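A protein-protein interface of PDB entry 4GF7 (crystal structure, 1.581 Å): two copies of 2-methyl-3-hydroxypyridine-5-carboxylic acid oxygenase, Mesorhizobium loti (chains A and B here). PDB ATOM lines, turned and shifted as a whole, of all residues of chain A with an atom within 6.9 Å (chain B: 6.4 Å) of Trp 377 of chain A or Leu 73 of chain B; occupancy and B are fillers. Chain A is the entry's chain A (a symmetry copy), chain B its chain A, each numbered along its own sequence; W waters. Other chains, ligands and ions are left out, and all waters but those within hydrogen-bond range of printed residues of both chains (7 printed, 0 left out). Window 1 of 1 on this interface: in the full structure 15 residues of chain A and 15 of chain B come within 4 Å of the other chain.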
ATOM      1  N   HIS A  57      20.390   7.339  21.396  1.00  0.00           N
ATOM      2  CA  HIS A  57      21.297   7.612  22.506  1.00  0.00           C
ATOM      3  C   HIS A  57      22.345   8.696  22.204  1.00  0.00           C
ATOM      4  O   HIS A  57      22.481   9.655  22.973  1.00  0.00           O
ATOM      5  CB  HIS A  57      21.950   6.294  22.944  1.00  0.00           C
ATOM      6  CG  HIS A  57      23.166   6.459  23.799  1.00  0.00           C
ATOM      7  ND1 HIS A  57      24.439   6.294  23.301  1.00  0.00           N
ATOM      8  CD2 HIS A  57      23.306   6.733  25.119  1.00  0.00           C
ATOM      9  CE1 HIS A  57      25.317   6.485  24.276  1.00  0.00           C
ATOM     10  NE2 HIS A  57      24.655   6.757  25.387  1.00  0.00           N
ATOM     11  N   ARG A  61      22.254  12.219  24.029  1.00  0.00           N
ATOM     12  CA  ARG A  61      23.367  12.635  24.869  1.00  0.00           C
ATOM     13  C   ARG A  61      23.863  14.018  24.461  1.00  0.00           C
ATOM     14  O   ARG A  61      24.225  14.813  25.326  1.00  0.00           O
ATOM     15  CB  ARG A  61      24.492  11.600  24.846  1.00  0.00           C
ATOM     16  CG  ARG A  61      24.134  10.317  25.604  1.00  0.00           C
ATOM     17  CD  ARG A  61      24.065  10.532  27.127  1.00  0.00           C
ATOM     18  NE  ARG A  61      25.406  10.569  27.707  1.00  0.00           N
ATOM     19  CZ  ARG A  61      25.658  10.606  29.011  1.00  0.00           C
ATOM     20  NH1 ARG A  61      24.660  10.637  29.887  1.00  0.00           N
ATOM     21  NH2 ARG A  61      26.912  10.605  29.435  1.00  0.00           N
ATOM     22  N   PHE A  96      16.673  -3.016  20.817  1.00  0.00           N
ATOM     23  CA  PHE A  96      18.048  -2.519  20.915  1.00  0.00           C
ATOM     24  C   PHE A  96      18.692  -2.674  22.298  1.00  0.00           C
ATOM     25  O   PHE A  96      19.548  -1.877  22.668  1.00  0.00           O
ATOM     26  CB  PHE A  96      18.120  -1.053  20.464  1.00  0.00           C
ATOM     27  CG  PHE A  96      17.213  -0.728  19.296  1.00  0.00           C
ATOM     28  CD1 PHE A  96      17.382  -1.353  18.070  1.00  0.00           C
ATOM     29  CD2 PHE A  96      16.202   0.215  19.431  1.00  0.00           C
ATOM     30  CE1 PHE A  96      16.550  -1.059  16.999  1.00  0.00           C
ATOM     31  CE2 PHE A  96      15.361   0.522  18.363  1.00  0.00           C
ATOM     32  CZ  PHE A  96      15.542  -0.113  17.145  1.00  0.00           C
ATOM     33  N   ASN A  97      18.285  -3.702  23.043  1.00  0.00           N
ATOM     34  CA  ASN A  97      18.848  -3.958  24.369  1.00  0.00           C
ATOM     35  C   ASN A  97      18.890  -2.704  25.242  1.00  0.00           C
ATOM     36  O   ASN A  97      19.902  -2.399  25.889  1.00  0.00           O
ATOM     37  CB  ASN A  97      20.235  -4.596  24.240  1.00  0.00           C
ATOM     38  CG  ASN A  97      20.194  -5.913  23.488  1.00  0.00           C
ATOM     39  OD1 ASN A  97      19.817  -6.944  24.056  1.00  0.00           O
ATOM     40  ND2 ASN A  97      20.576  -5.892  22.202  1.00  0.00           N
ATOM     41  N   GLY A  98      17.792  -1.953  25.219  1.00  0.00           N
ATOM     42  CA  GLY A  98      17.628  -0.824  26.112  1.00  0.00           C
ATOM     43  C   GLY A  98      18.239   0.484  25.648  1.00  0.00           C
ATOM     44  O   GLY A  98      18.090   1.492  26.336  1.00  0.00           O
ATOM     45  N   LEU A  99      18.930   0.471  24.508  1.00  0.00           N
ATOM     46  CA  LEU A  99      19.529   1.687  23.967  1.00  0.00           C
ATOM     47  C   LEU A  99      18.449   2.762  23.787  1.00  0.00           C
ATOM     48  O   LEU A  99      17.449   2.528  23.108  1.00  0.00           O
ATOM     49  CB  LEU A  99      20.227   1.384  22.638  1.00  0.00           C
ATOM     50  CG  LEU A  99      21.089   2.495  22.042  1.00  0.00           C
ATOM     51  CD1 LEU A  99      22.279   1.882  21.326  1.00  0.00           C
ATOM     52  CD2 LEU A  99      20.297   3.341  21.096  1.00  0.00           C
ATOM     53  N   PRO A 100      18.638   3.940  24.407  1.00  0.00           N
ATOM     54  CA  PRO A 100      17.594   4.972  24.325  1.00  0.00           C
ATOM     55  C   PRO A 100      17.367   5.483  22.903  1.00  0.00           C
ATOM     56  O   PRO A 100      18.316   5.608  22.124  1.00  0.00           O
ATOM     57  CB  PRO A 100      18.136   6.086  25.224  1.00  0.00           C
ATOM     58  CG  PRO A 100      18.993   5.347  26.239  1.00  0.00           C
ATOM     59  CD  PRO A 100      19.647   4.252  25.435  1.00  0.00           C
ATOM     60  N   LEU A 363      24.274  -0.160  14.783  1.00  0.00           N
ATOM     61  CA  LEU A 363      24.021   0.723  15.926  1.00  0.00           C
ATOM     62  C   LEU A 363      25.260   1.425  16.472  1.00  0.00           C
ATOM     63  O   LEU A 363      25.182   2.097  17.511  1.00  0.00           O
ATOM     64  CB  LEU A 363      23.353  -0.065  17.056  1.00  0.00           C
ATOM     65  CG  LEU A 363      21.917  -0.502  16.794  1.00  0.00           C
ATOM     66  CD1 LEU A 363      21.463  -1.469  17.882  1.00  0.00           C
ATOM     67  CD2 LEU A 363      20.987   0.697  16.720  1.00  0.00           C
ATOM     68  N   ALA A 366      24.798   5.161  17.067  1.00  0.00           N
ATOM     69  CA  ALA A 366      23.827   5.342  18.139  1.00  0.00           C
ATOM     70  C   ALA A 366      24.427   5.049  19.512  1.00  0.00           C
ATOM     71  O   ALA A 366      24.067   5.696  20.506  1.00  0.00           O
ATOM     72  CB  ALA A 366      22.616   4.452  17.895  1.00  0.00           C
ATOM     73  N   ARG A 367      25.328   4.066  19.561  1.00  0.00           N
ATOM     74  CA  ARG A 367      25.951   3.627  20.810  1.00  0.00           C
ATOM     75  C   ARG A 367      26.988   4.601  21.339  1.00  0.00           C
ATOM     76  O   ARG A 367      27.289   4.599  22.534  1.00  0.00           O
ATOM     77  CB  ARG A 367      26.603   2.254  20.623  1.00  0.00           C
ATOM     78  CG  ARG A 367      25.605   1.122  20.378  1.00  0.00           C
ATOM     79  CD  ARG A 367      26.295  -0.233  20.313  1.00  0.00           C
ATOM     80  NE  ARG A 367      27.015  -0.444  21.560  1.00  0.00           N
ATOM     81  CZ  ARG A 367      28.330  -0.593  21.654  1.00  0.00           C
ATOM     82  NH1 ARG A 367      29.086  -0.601  20.558  1.00  0.00           N
ATOM     83  NH2 ARG A 367      28.883  -0.740  22.852  1.00  0.00           N
ATOM     84  N   TYR A 375      31.746   4.124  23.957  1.00  0.00           N
ATOM     85  CA  TYR A 375      30.548   3.463  23.455  1.00  0.00           C
ATOM     86  C   TYR A 375      29.797   2.850  24.626  1.00  0.00           C
ATOM     87  O   TYR A 375      30.402   2.236  25.508  1.00  0.00           O
ATOM     88  CB  TYR A 375      30.905   2.402  22.409  1.00  0.00           C
ATOM     89  CG  TYR A 375      31.455   2.988  21.129  1.00  0.00           C
ATOM     90  CD1 TYR A 375      32.813   3.224  20.977  1.00  0.00           C
ATOM     91  CD2 TYR A 375      30.612   3.318  20.077  1.00  0.00           C
ATOM     92  CE1 TYR A 375      33.317   3.771  19.805  1.00  0.00           C
ATOM     93  CE2 TYR A 375      31.109   3.861  18.902  1.00  0.00           C
ATOM     94  CZ  TYR A 375      32.459   4.082  18.772  1.00  0.00           C
ATOM     95  OH  TYR A 375      32.962   4.621  17.599  1.00  0.00           O
ATOM     96  N   SER A 376      28.480   3.039  24.642  1.00  0.00           N
ATOM     97  CA  SER A 376      27.651   2.526  25.733  1.00  0.00           C
ATOM     98  C   SER A 376      26.599   1.575  25.158  1.00  0.00           C
ATOM     99  O   SER A 376      26.707   1.169  24.001  1.00  0.00           O
ATOM    100  CB  SER A 376      27.020   3.696  26.500  1.00  0.00           C
ATOM    101  OG  SER A 376      26.360   3.277  27.682  1.00  0.00           O
ATOM    102  N   TRP A 377      25.613   1.194  25.969  1.00  0.00           N
ATOM    103  CA  TRP A 377      24.511   0.315  25.532  1.00  0.00           C
ATOM    104  C   TRP A 377      24.936  -0.837  24.612  1.00  0.00           C
ATOM    105  O   TRP A 377      24.536  -0.905  23.443  1.00  0.00           O
ATOM    106  CB  TRP A 377      23.384   1.170  24.934  1.00  0.00           C
ATOM    107  CG  TRP A 377      22.888   2.136  25.965  1.00  0.00           C
ATOM    108  CD1 TRP A 377      23.227   3.456  26.101  1.00  0.00           C
ATOM    109  CD2 TRP A 377      22.017   1.832  27.057  1.00  0.00           C
ATOM    110  NE1 TRP A 377      22.597   3.993  27.201  1.00  0.00           N
ATOM    111  CE2 TRP A 377      21.853   3.013  27.808  1.00  0.00           C
ATOM    112  CE3 TRP A 377      21.364   0.671  27.478  1.00  0.00           C
ATOM    113  CZ2 TRP A 377      21.047   3.065  28.951  1.00  0.00           C
ATOM    114  CZ3 TRP A 377      20.564   0.723  28.604  1.00  0.00           C
ATOM    115  CH2 TRP A 377      20.412   1.912  29.330  1.00  0.00           C
ATOM    116  N   PRO A 378      25.769  -1.750  25.137  1.00  0.00           N
ATOM    117  CA  PRO A 378      26.287  -2.872  24.343  1.00  0.00           C
ATOM    118  C   PRO A 378      25.196  -3.808  23.846  1.00  0.00           C
ATOM    119  O   PRO A 378      24.163  -3.984  24.494  1.00  0.00           O
ATOM    120  CB  PRO A 378      27.217  -3.597  25.322  1.00  0.00           C
ATOM    121  CG  PRO A 378      26.722  -3.204  26.678  1.00  0.00           C
ATOM    122  CD  PRO A 378      26.273  -1.783  26.524  1.00  0.00           C
ATOM    123  N   GLN A 379      25.449  -4.411  22.687  1.00  0.00           N
ATOM    124  CA  GLN A 379      24.448  -5.205  21.993  1.00  0.00           C
ATOM    125  C   GLN A 379      24.811  -6.686  21.982  1.00  0.00           C
ATOM    126  O   GLN A 379      25.809  -7.101  22.577  1.00  0.00           O
ATOM    127  CB  GLN A 379      24.304  -4.697  20.555  1.00  0.00           C
ATOM    128  CG  GLN A 379      23.878  -3.244  20.468  1.00  0.00           C
ATOM    129  CD  GLN A 379      22.470  -3.039  20.983  1.00  0.00           C
ATOM    130  OE1 GLN A 379      21.545  -3.717  20.555  1.00  0.00           O
ATOM    131  NE2 GLN A 379      22.307  -2.123  21.927  1.00  0.00           N
ATOM    132  OXT GLN A 379      24.112  -7.501  21.373  1.00  0.00           O
ATOM    133  N   LEU B  60      20.667   3.868  37.376  1.00  0.00           N
ATOM    134  CA  LEU B  60      21.625   3.849  36.276  1.00  0.00           C
ATOM    135  C   LEU B  60      22.383   5.167  36.211  1.00  0.00           C
ATOM    136  O   LEU B  60      23.563   5.194  35.874  1.00  0.00           O
ATOM    137  CB  LEU B  60      20.912   3.567  34.950  1.00  0.00           C
ATOM    138  CG  LEU B  60      20.266   2.190  34.881  1.00  0.00           C
ATOM    139  CD1 LEU B  60      19.391   2.096  33.635  1.00  0.00           C
ATOM    140  CD2 LEU B  60      21.315   1.106  34.872  1.00  0.00           C
ATOM    141  N   ALA B  68      30.685   3.506  37.172  1.00  0.00           N
ATOM    142  CA  ALA B  68      30.514   2.055  37.241  1.00  0.00           C
ATOM    143  C   ALA B  68      29.440   1.557  36.280  1.00  0.00           C
ATOM    144  O   ALA B  68      29.057   0.390  36.324  1.00  0.00           O
ATOM    145  CB  ALA B  68      30.180   1.641  38.659  1.00  0.00           C
ATOM    146  N   LEU B  69      28.960   2.442  35.412  1.00  0.00           N
ATOM    147  CA  LEU B  69      27.872   2.085  34.507  1.00  0.00           C
ATOM    148  C   LEU B  69      28.300   1.106  33.414  1.00  0.00           C
ATOM    149  O   LEU B  69      27.542   0.188  33.091  1.00  0.00           O
ATOM    150  CB  LEU B  69      27.245   3.331  33.874  1.00  0.00           C
ATOM    151  CG  LEU B  69      26.120   3.068  32.868  1.00  0.00           C
ATOM    152  CD1 LEU B  69      24.878   2.532  33.578  1.00  0.00           C
ATOM    153  CD2 LEU B  69      25.822   4.336  32.083  1.00  0.00           C
ATOM    154  N   ASP B  70      29.493   1.302  32.844  1.00  0.00           N
ATOM    155  CA  ASP B  70      29.934   0.468  31.721  1.00  0.00           C
ATOM    156  C   ASP B  70      29.971  -1.015  32.079  1.00  0.00           C
ATOM    157  O   ASP B  70      29.496  -1.858  31.313  1.00  0.00           O
ATOM    158  CB  ASP B  70      31.311   0.910  31.201  1.00  0.00           C
ATOM    159  CG  ASP B  70      31.319   2.345  30.692  1.00  0.00           C
ATOM    160  OD1 ASP B  70      30.261   2.840  30.257  1.00  0.00           O
ATOM    161  OD2 ASP B  70      32.399   2.978  30.727  1.00  0.00           O
ATOM    162  N   ASP B  71      30.532  -1.326  33.246  1.00  0.00           N
ATOM    163  CA  ASP B  71      30.668  -2.707  33.693  1.00  0.00           C
ATOM    164  C   ASP B  71      29.310  -3.322  34.030  1.00  0.00           C
ATOM    165  O   ASP B  71      29.148  -4.543  33.994  1.00  0.00           O
ATOM    166  CB  ASP B  71      31.577  -2.798  34.929  1.00  0.00           C
ATOM    167  CG  ASP B  71      33.048  -2.666  34.591  1.00  0.00           C
ATOM    168  OD1 ASP B  71      33.415  -2.780  33.400  1.00  0.00           O
ATOM    169  OD2 ASP B  71      33.846  -2.461  35.533  1.00  0.00           O
ATOM    170  N   VAL B  72      28.343  -2.478  34.381  1.00  0.00           N
ATOM    171  CA  VAL B  72      26.995  -2.959  34.654  1.00  0.00           C
ATOM    172  C   VAL B  72      26.229  -3.256  33.356  1.00  0.00           C
ATOM    173  O   VAL B  72      25.664  -4.330  33.210  1.00  0.00           O
ATOM    174  CB  VAL B  72      26.203  -1.991  35.557  1.00  0.00           C
ATOM    175  CG1 VAL B  72      24.741  -2.383  35.603  1.00  0.00           C
ATOM    176  CG2 VAL B  72      26.784  -1.992  36.962  1.00  0.00           C
ATOM    177  N   LEU B  73      26.220  -2.323  32.408  1.00  0.00           N
ATOM    178  CA  LEU B  73      25.447  -2.539  31.189  1.00  0.00           C
ATOM    179  C   LEU B  73      25.972  -3.720  30.379  1.00  0.00           C
ATOM    180  O   LEU B  73      25.195  -4.494  29.819  1.00  0.00           O
ATOM    181  CB  LEU B  73      25.402  -1.272  30.331  1.00  0.00           C
ATOM    182  CG  LEU B  73      24.695  -0.059  30.926  1.00  0.00           C
ATOM    183  CD1 LEU B  73      24.689   1.045  29.876  1.00  0.00           C
ATOM    184  CD2 LEU B  73      23.265  -0.380  31.375  1.00  0.00           C
ATOM    185  N   GLN B  74      27.291  -3.860  30.312  1.00  0.00           N
ATOM    186  CA  GLN B  74      27.876  -5.037  29.702  1.00  0.00           C
ATOM    187  C   GLN B  74      27.538  -6.269  30.529  1.00  0.00           C
ATOM    188  O   GLN B  74      27.938  -6.372  31.692  1.00  0.00           O
ATOM    189  CB  GLN B  74      29.394  -4.869  29.612  1.00  0.00           C
ATOM    190  CG  GLN B  74      30.094  -6.012  28.891  1.00  0.00           C
ATOM    191  CD  GLN B  74      29.759  -6.064  27.405  1.00  0.00           C
ATOM    192  OE1 GLN B  74      29.859  -5.063  26.692  1.00  0.00           O
ATOM    193  NE2 GLN B  74      29.359  -7.238  26.937  1.00  0.00           N
ATOM    194  N   GLY B  75      26.774  -7.188  29.954  1.00  0.00           N
ATOM    195  CA  GLY B  75      26.426  -8.412  30.663  1.00  0.00           C
ATOM    196  C   GLY B  75      25.142  -8.366  31.478  1.00  0.00           C
ATOM    197  O   GLY B  75      24.890  -9.263  32.290  1.00  0.00           O
ATOM    198  N   SER B  76      24.335  -7.329  31.260  1.00  0.00           N
ATOM    199  CA  SER B  76      23.001  -7.251  31.852  1.00  0.00           C
ATOM    200  C   SER B  76      21.971  -7.055  30.736  1.00  0.00           C
ATOM    201  O   SER B  76      22.331  -7.062  29.556  1.00  0.00           O
ATOM    202  CB  SER B  76      22.923  -6.131  32.894  1.00  0.00           C
ATOM    203  OG  SER B  76      23.210  -4.871  32.312  1.00  0.00           O
ATOM    204  N   HIS B  77      20.706  -6.860  31.093  1.00  0.00           N
ATOM    205  CA  HIS B  77      19.617  -7.029  30.124  1.00  0.00           C
ATOM    206  C   HIS B  77      18.529  -5.979  30.304  1.00  0.00           C
ATOM    207  O   HIS B  77      18.122  -5.702  31.428  1.00  0.00           O
ATOM    208  CB  HIS B  77      19.033  -8.432  30.347  1.00  0.00           C
ATOM    209  CG  HIS B  77      17.866  -8.796  29.475  1.00  0.00           C
ATOM    210  ND1 HIS B  77      17.993  -9.072  28.131  1.00  0.00           N
ATOM    211  CD2 HIS B  77      16.567  -9.015  29.785  1.00  0.00           C
ATOM    212  CE1 HIS B  77      16.811  -9.417  27.643  1.00  0.00           C
ATOM    213  NE2 HIS B  77      15.928  -9.386  28.624  1.00  0.00           N
ATOM    214  N   THR B  78      18.056  -5.387  29.205  1.00  0.00           N
ATOM    215  CA  THR B  78      16.791  -4.659  29.258  1.00  0.00           C
ATOM    216  C   THR B  78      15.769  -5.438  28.452  1.00  0.00           C
ATOM    217  O   THR B  78      15.887  -5.547  27.226  1.00  0.00           O
ATOM    218  CB  THR B  78      16.872  -3.237  28.658  1.00  0.00           C
ATOM    219  OG1 THR B  78      17.879  -2.470  29.324  1.00  0.00           O
ATOM    220  CG2 THR B  78      15.528  -2.519  28.803  1.00  0.00           C
ATOM    221  N   PRO B 100      14.876   4.437  30.924  1.00  0.00           N
ATOM    222  CA  PRO B 100      15.840   3.329  30.966  1.00  0.00           C
ATOM    223  C   PRO B 100      15.657   2.422  32.182  1.00  0.00           C
ATOM    224  O   PRO B 100      15.328   2.895  33.272  1.00  0.00           O
ATOM    225  CB  PRO B 100      17.192   4.046  31.020  1.00  0.00           C
ATOM    226  CG  PRO B 100      16.932   5.361  30.306  1.00  0.00           C
ATOM    227  CD  PRO B 100      15.538   5.741  30.737  1.00  0.00           C
ATOM    228  N   TRP B 101      15.839   1.120  31.985  1.00  0.00           N
ATOM    229  CA  TRP B 101      15.812   0.173  33.101  1.00  0.00           C
ATOM    230  C   TRP B 101      16.670  -1.030  32.743  1.00  0.00           C
ATOM    231  O   TRP B 101      17.096  -1.169  31.594  1.00  0.00           O
ATOM    232  CB  TRP B 101      14.378  -0.236  33.470  1.00  0.00           C
ATOM    233  CG  TRP B 101      13.577  -0.889  32.387  1.00  0.00           C
ATOM    234  CD1 TRP B 101      13.212  -0.348  31.182  1.00  0.00           C
ATOM    235  CD2 TRP B 101      13.003  -2.196  32.430  1.00  0.00           C
ATOM    236  NE1 TRP B 101      12.448  -1.246  30.472  1.00  0.00           N
ATOM    237  CE2 TRP B 101      12.302  -2.390  31.219  1.00  0.00           C
ATOM    238  CE3 TRP B 101      13.004  -3.224  33.383  1.00  0.00           C
ATOM    239  CZ2 TRP B 101      11.621  -3.573  30.930  1.00  0.00           C
ATOM    240  CZ3 TRP B 101      12.329  -4.396  33.096  1.00  0.00           C
ATOM    241  CH2 TRP B 101      11.644  -4.564  31.882  1.00  0.00           C
ATOM    242  N   ARG B 102      16.945  -1.884  33.723  1.00  0.00           N
ATOM    243  CA  ARG B 102      17.924  -2.942  33.516  1.00  0.00           C
ATOM    244  C   ARG B 102      17.737  -4.035  34.557  1.00  0.00           C
ATOM    245  O   ARG B 102      17.396  -3.756  35.711  1.00  0.00           O
ATOM    246  CB  ARG B 102      19.343  -2.375  33.634  1.00  0.00           C
ATOM    247  CG  ARG B 102      20.403  -3.205  32.911  1.00  0.00           C
ATOM    248  CD  ARG B 102      20.238  -3.065  31.405  1.00  0.00           C
ATOM    249  NE  ARG B 102      21.424  -3.500  30.684  1.00  0.00           N
ATOM    250  CZ  ARG B 102      21.571  -3.378  29.371  1.00  0.00           C
ATOM    251  NH1 ARG B 102      20.584  -2.854  28.643  1.00  0.00           N
ATOM    252  NH2 ARG B 102      22.697  -3.775  28.786  1.00  0.00           N
ATOM    253  N   HIS B 108      26.559  -9.384  39.637  1.00  0.00           N
ATOM    254  CA  HIS B 108      26.993  -8.527  38.545  1.00  0.00           C
ATOM    255  C   HIS B 108      27.092  -7.066  38.978  1.00  0.00           C
ATOM    256  O   HIS B 108      28.079  -6.386  38.699  1.00  0.00           O
ATOM    257  CB  HIS B 108      26.028  -8.667  37.365  1.00  0.00           C
ATOM    258  CG  HIS B 108      26.510  -8.008  36.115  1.00  0.00           C
ATOM    259  ND1 HIS B 108      27.513  -8.548  35.334  1.00  0.00           N
ATOM    260  CD2 HIS B 108      26.140  -6.857  35.506  1.00  0.00           C
ATOM    261  CE1 HIS B 108      27.732  -7.759  34.300  1.00  0.00           C
ATOM    262  NE2 HIS B 108      26.913  -6.723  34.379  1.00  0.00           N
HETATM  263  O   HOH W   1      19.228  -6.565  26.748  1.00  0.00           O
HETATM  264  O   HOH W   2      16.533   0.960  28.788  1.00  0.00           O
HETATM  265  O   HOH W   3      27.410  -7.472  24.775  1.00  0.00           O
HETATM  266  O   HOH W   4      22.667  -2.381  26.075  1.00  0.00           O
HETATM  267  O   HOH W   5      15.314  -3.640  25.181  1.00  0.00           O
HETATM  268  O   HOH W   6      32.308   2.118  27.529  1.00  0.00           O
HETATM  269  O   HOH W   7      28.137   1.931  29.137  1.00  0.00           O
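Water W7 bridges the side-chain carboxylate of Asp 70 of chain B (2.6 Å) and the side-chain hydroxyl of Ser 376 of chain A (2.7 Å). Water W4 lies within hydrogen-bond range of O of Pro 378 of chain A (2.7 Å), O of Asn 97 of chain A (2.8 Å) and NH2 of Arg 102 of chain B (3.0 Å). Water W3 bridges the chain-end carboxylate (O) of Gln 379 of chain A (2.7 Å) and the side-chain amide nitrogen (NE2) of Gln 74 of chain B (2.9 Å). Water W6 lies within hydrogen-bond range of the backbone carbonyl oxygen of Tyr 375 of chain A (2.8 Å) and the side-chain carboxylate of Asp 70 of chain B (3.3 Å). Water W1 lies within hydrogen-bond range of the side-chain amide oxygen of Asn 97 of chain A (2.8 Å), the backbone NH of Thr 78 of chain B (3.0 Å) and a ring nitrogen (ND1) of His 77 of chain B (3.1 Å). Water W5 lies within hydrogen-bond range of the backbone carbonyl oxygen of Thr 78 of chain B (2.9 Å) and the backbone NH of Gly 98 of chain A (3.0 Å).
The guanidinium group (NH1) of Arg 102 of chain B sits at hydrogen-bond distance from the backbone carbonyl oxygen (O) of Asn 97 of chain A.
OG of Ser 76 of chain B sits at hydrogen-bond distance from O of Leu 73 of chain B, 3.2 Å away. The guanidinium group (NH2) of Arg 102 of chain B sits at hydrogen-bond distance from the backbone carbonyl oxygen (O) of Leu 73 of chain B. The side-chain hydroxyl (OG) of Ser 76 of chain B lies within hydrogen-bond range of the guanidinium group (NE) of Arg 102 of chain B (2.8 Å). The side-chain hydroxyl of Thr 78 of chain B is in hydrogen-bond range of the backbone carbonyl oxygen of Trp 101 of chain B, 2.7 Å away. The backbone NH (N) of Ser 376 of chain A is in hydrogen-bond range of the backbone carbonyl oxygen (O) of Arg 367 of chain A, at 2.9 Å. The backbone carbonyl oxygen (O) of Trp 377 of chain A sits at hydrogen-bond distance from the guanidinium group (NE) of Arg 367 of chain A (3.1 Å).
Among the printed residues, pairs that only touch across the chains: Pro 378 of chain A with Gln 74 of chain B, Ser 376 of chain A with Leu 73 of chain B, Trp 377 of chain A with Arg 102 of chain B, Gly 98 of chain A with Thr 78 of chain B, Pro 378 of chain A with Leu 73 of chain B, Trp 377 of chain A with Leu 73 of chain B and Asn 97 of chain A with Thr 78 of chain B.
Of chain B, only Leu 73 (3.96 Å) and Arg 102 (3.6 Å) come within 4 Å of Trp 377 of chain A. Leu 73 of chain B touches just these residues of chain A: Ser 376, Trp 377 and Pro 378. Printed residues of chain A within 4 Å of Thr 78 of chain B: Asn 97 (3.99 Å) and Gly 98 (3.6 Å). Printed residues of chain B within 4 Å of Ser 376 of chain A: Leu 73. Of the printed residues of chain A, Gln 74 of chain B touches Pro 378 (3.3 Å). Printed residues of chain B within 4 Å of Gly 98 of chain A: Thr 78 (3.6 Å). Printed residues of chain B within 4 Å of Asn 97 of chain A: Thr 78 (3.99 Å) and Arg 102 (2.9 Å). The nearest printed residue of chain B that does not touch Trp 377 of chain A is Pro 100 of chain B (4.2 Å). The nearest printed residue of chain A that does not touch Thr 78 of chain B is Trp 377 of chain A (4.2 Å).
Position printed for both chains: 100.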
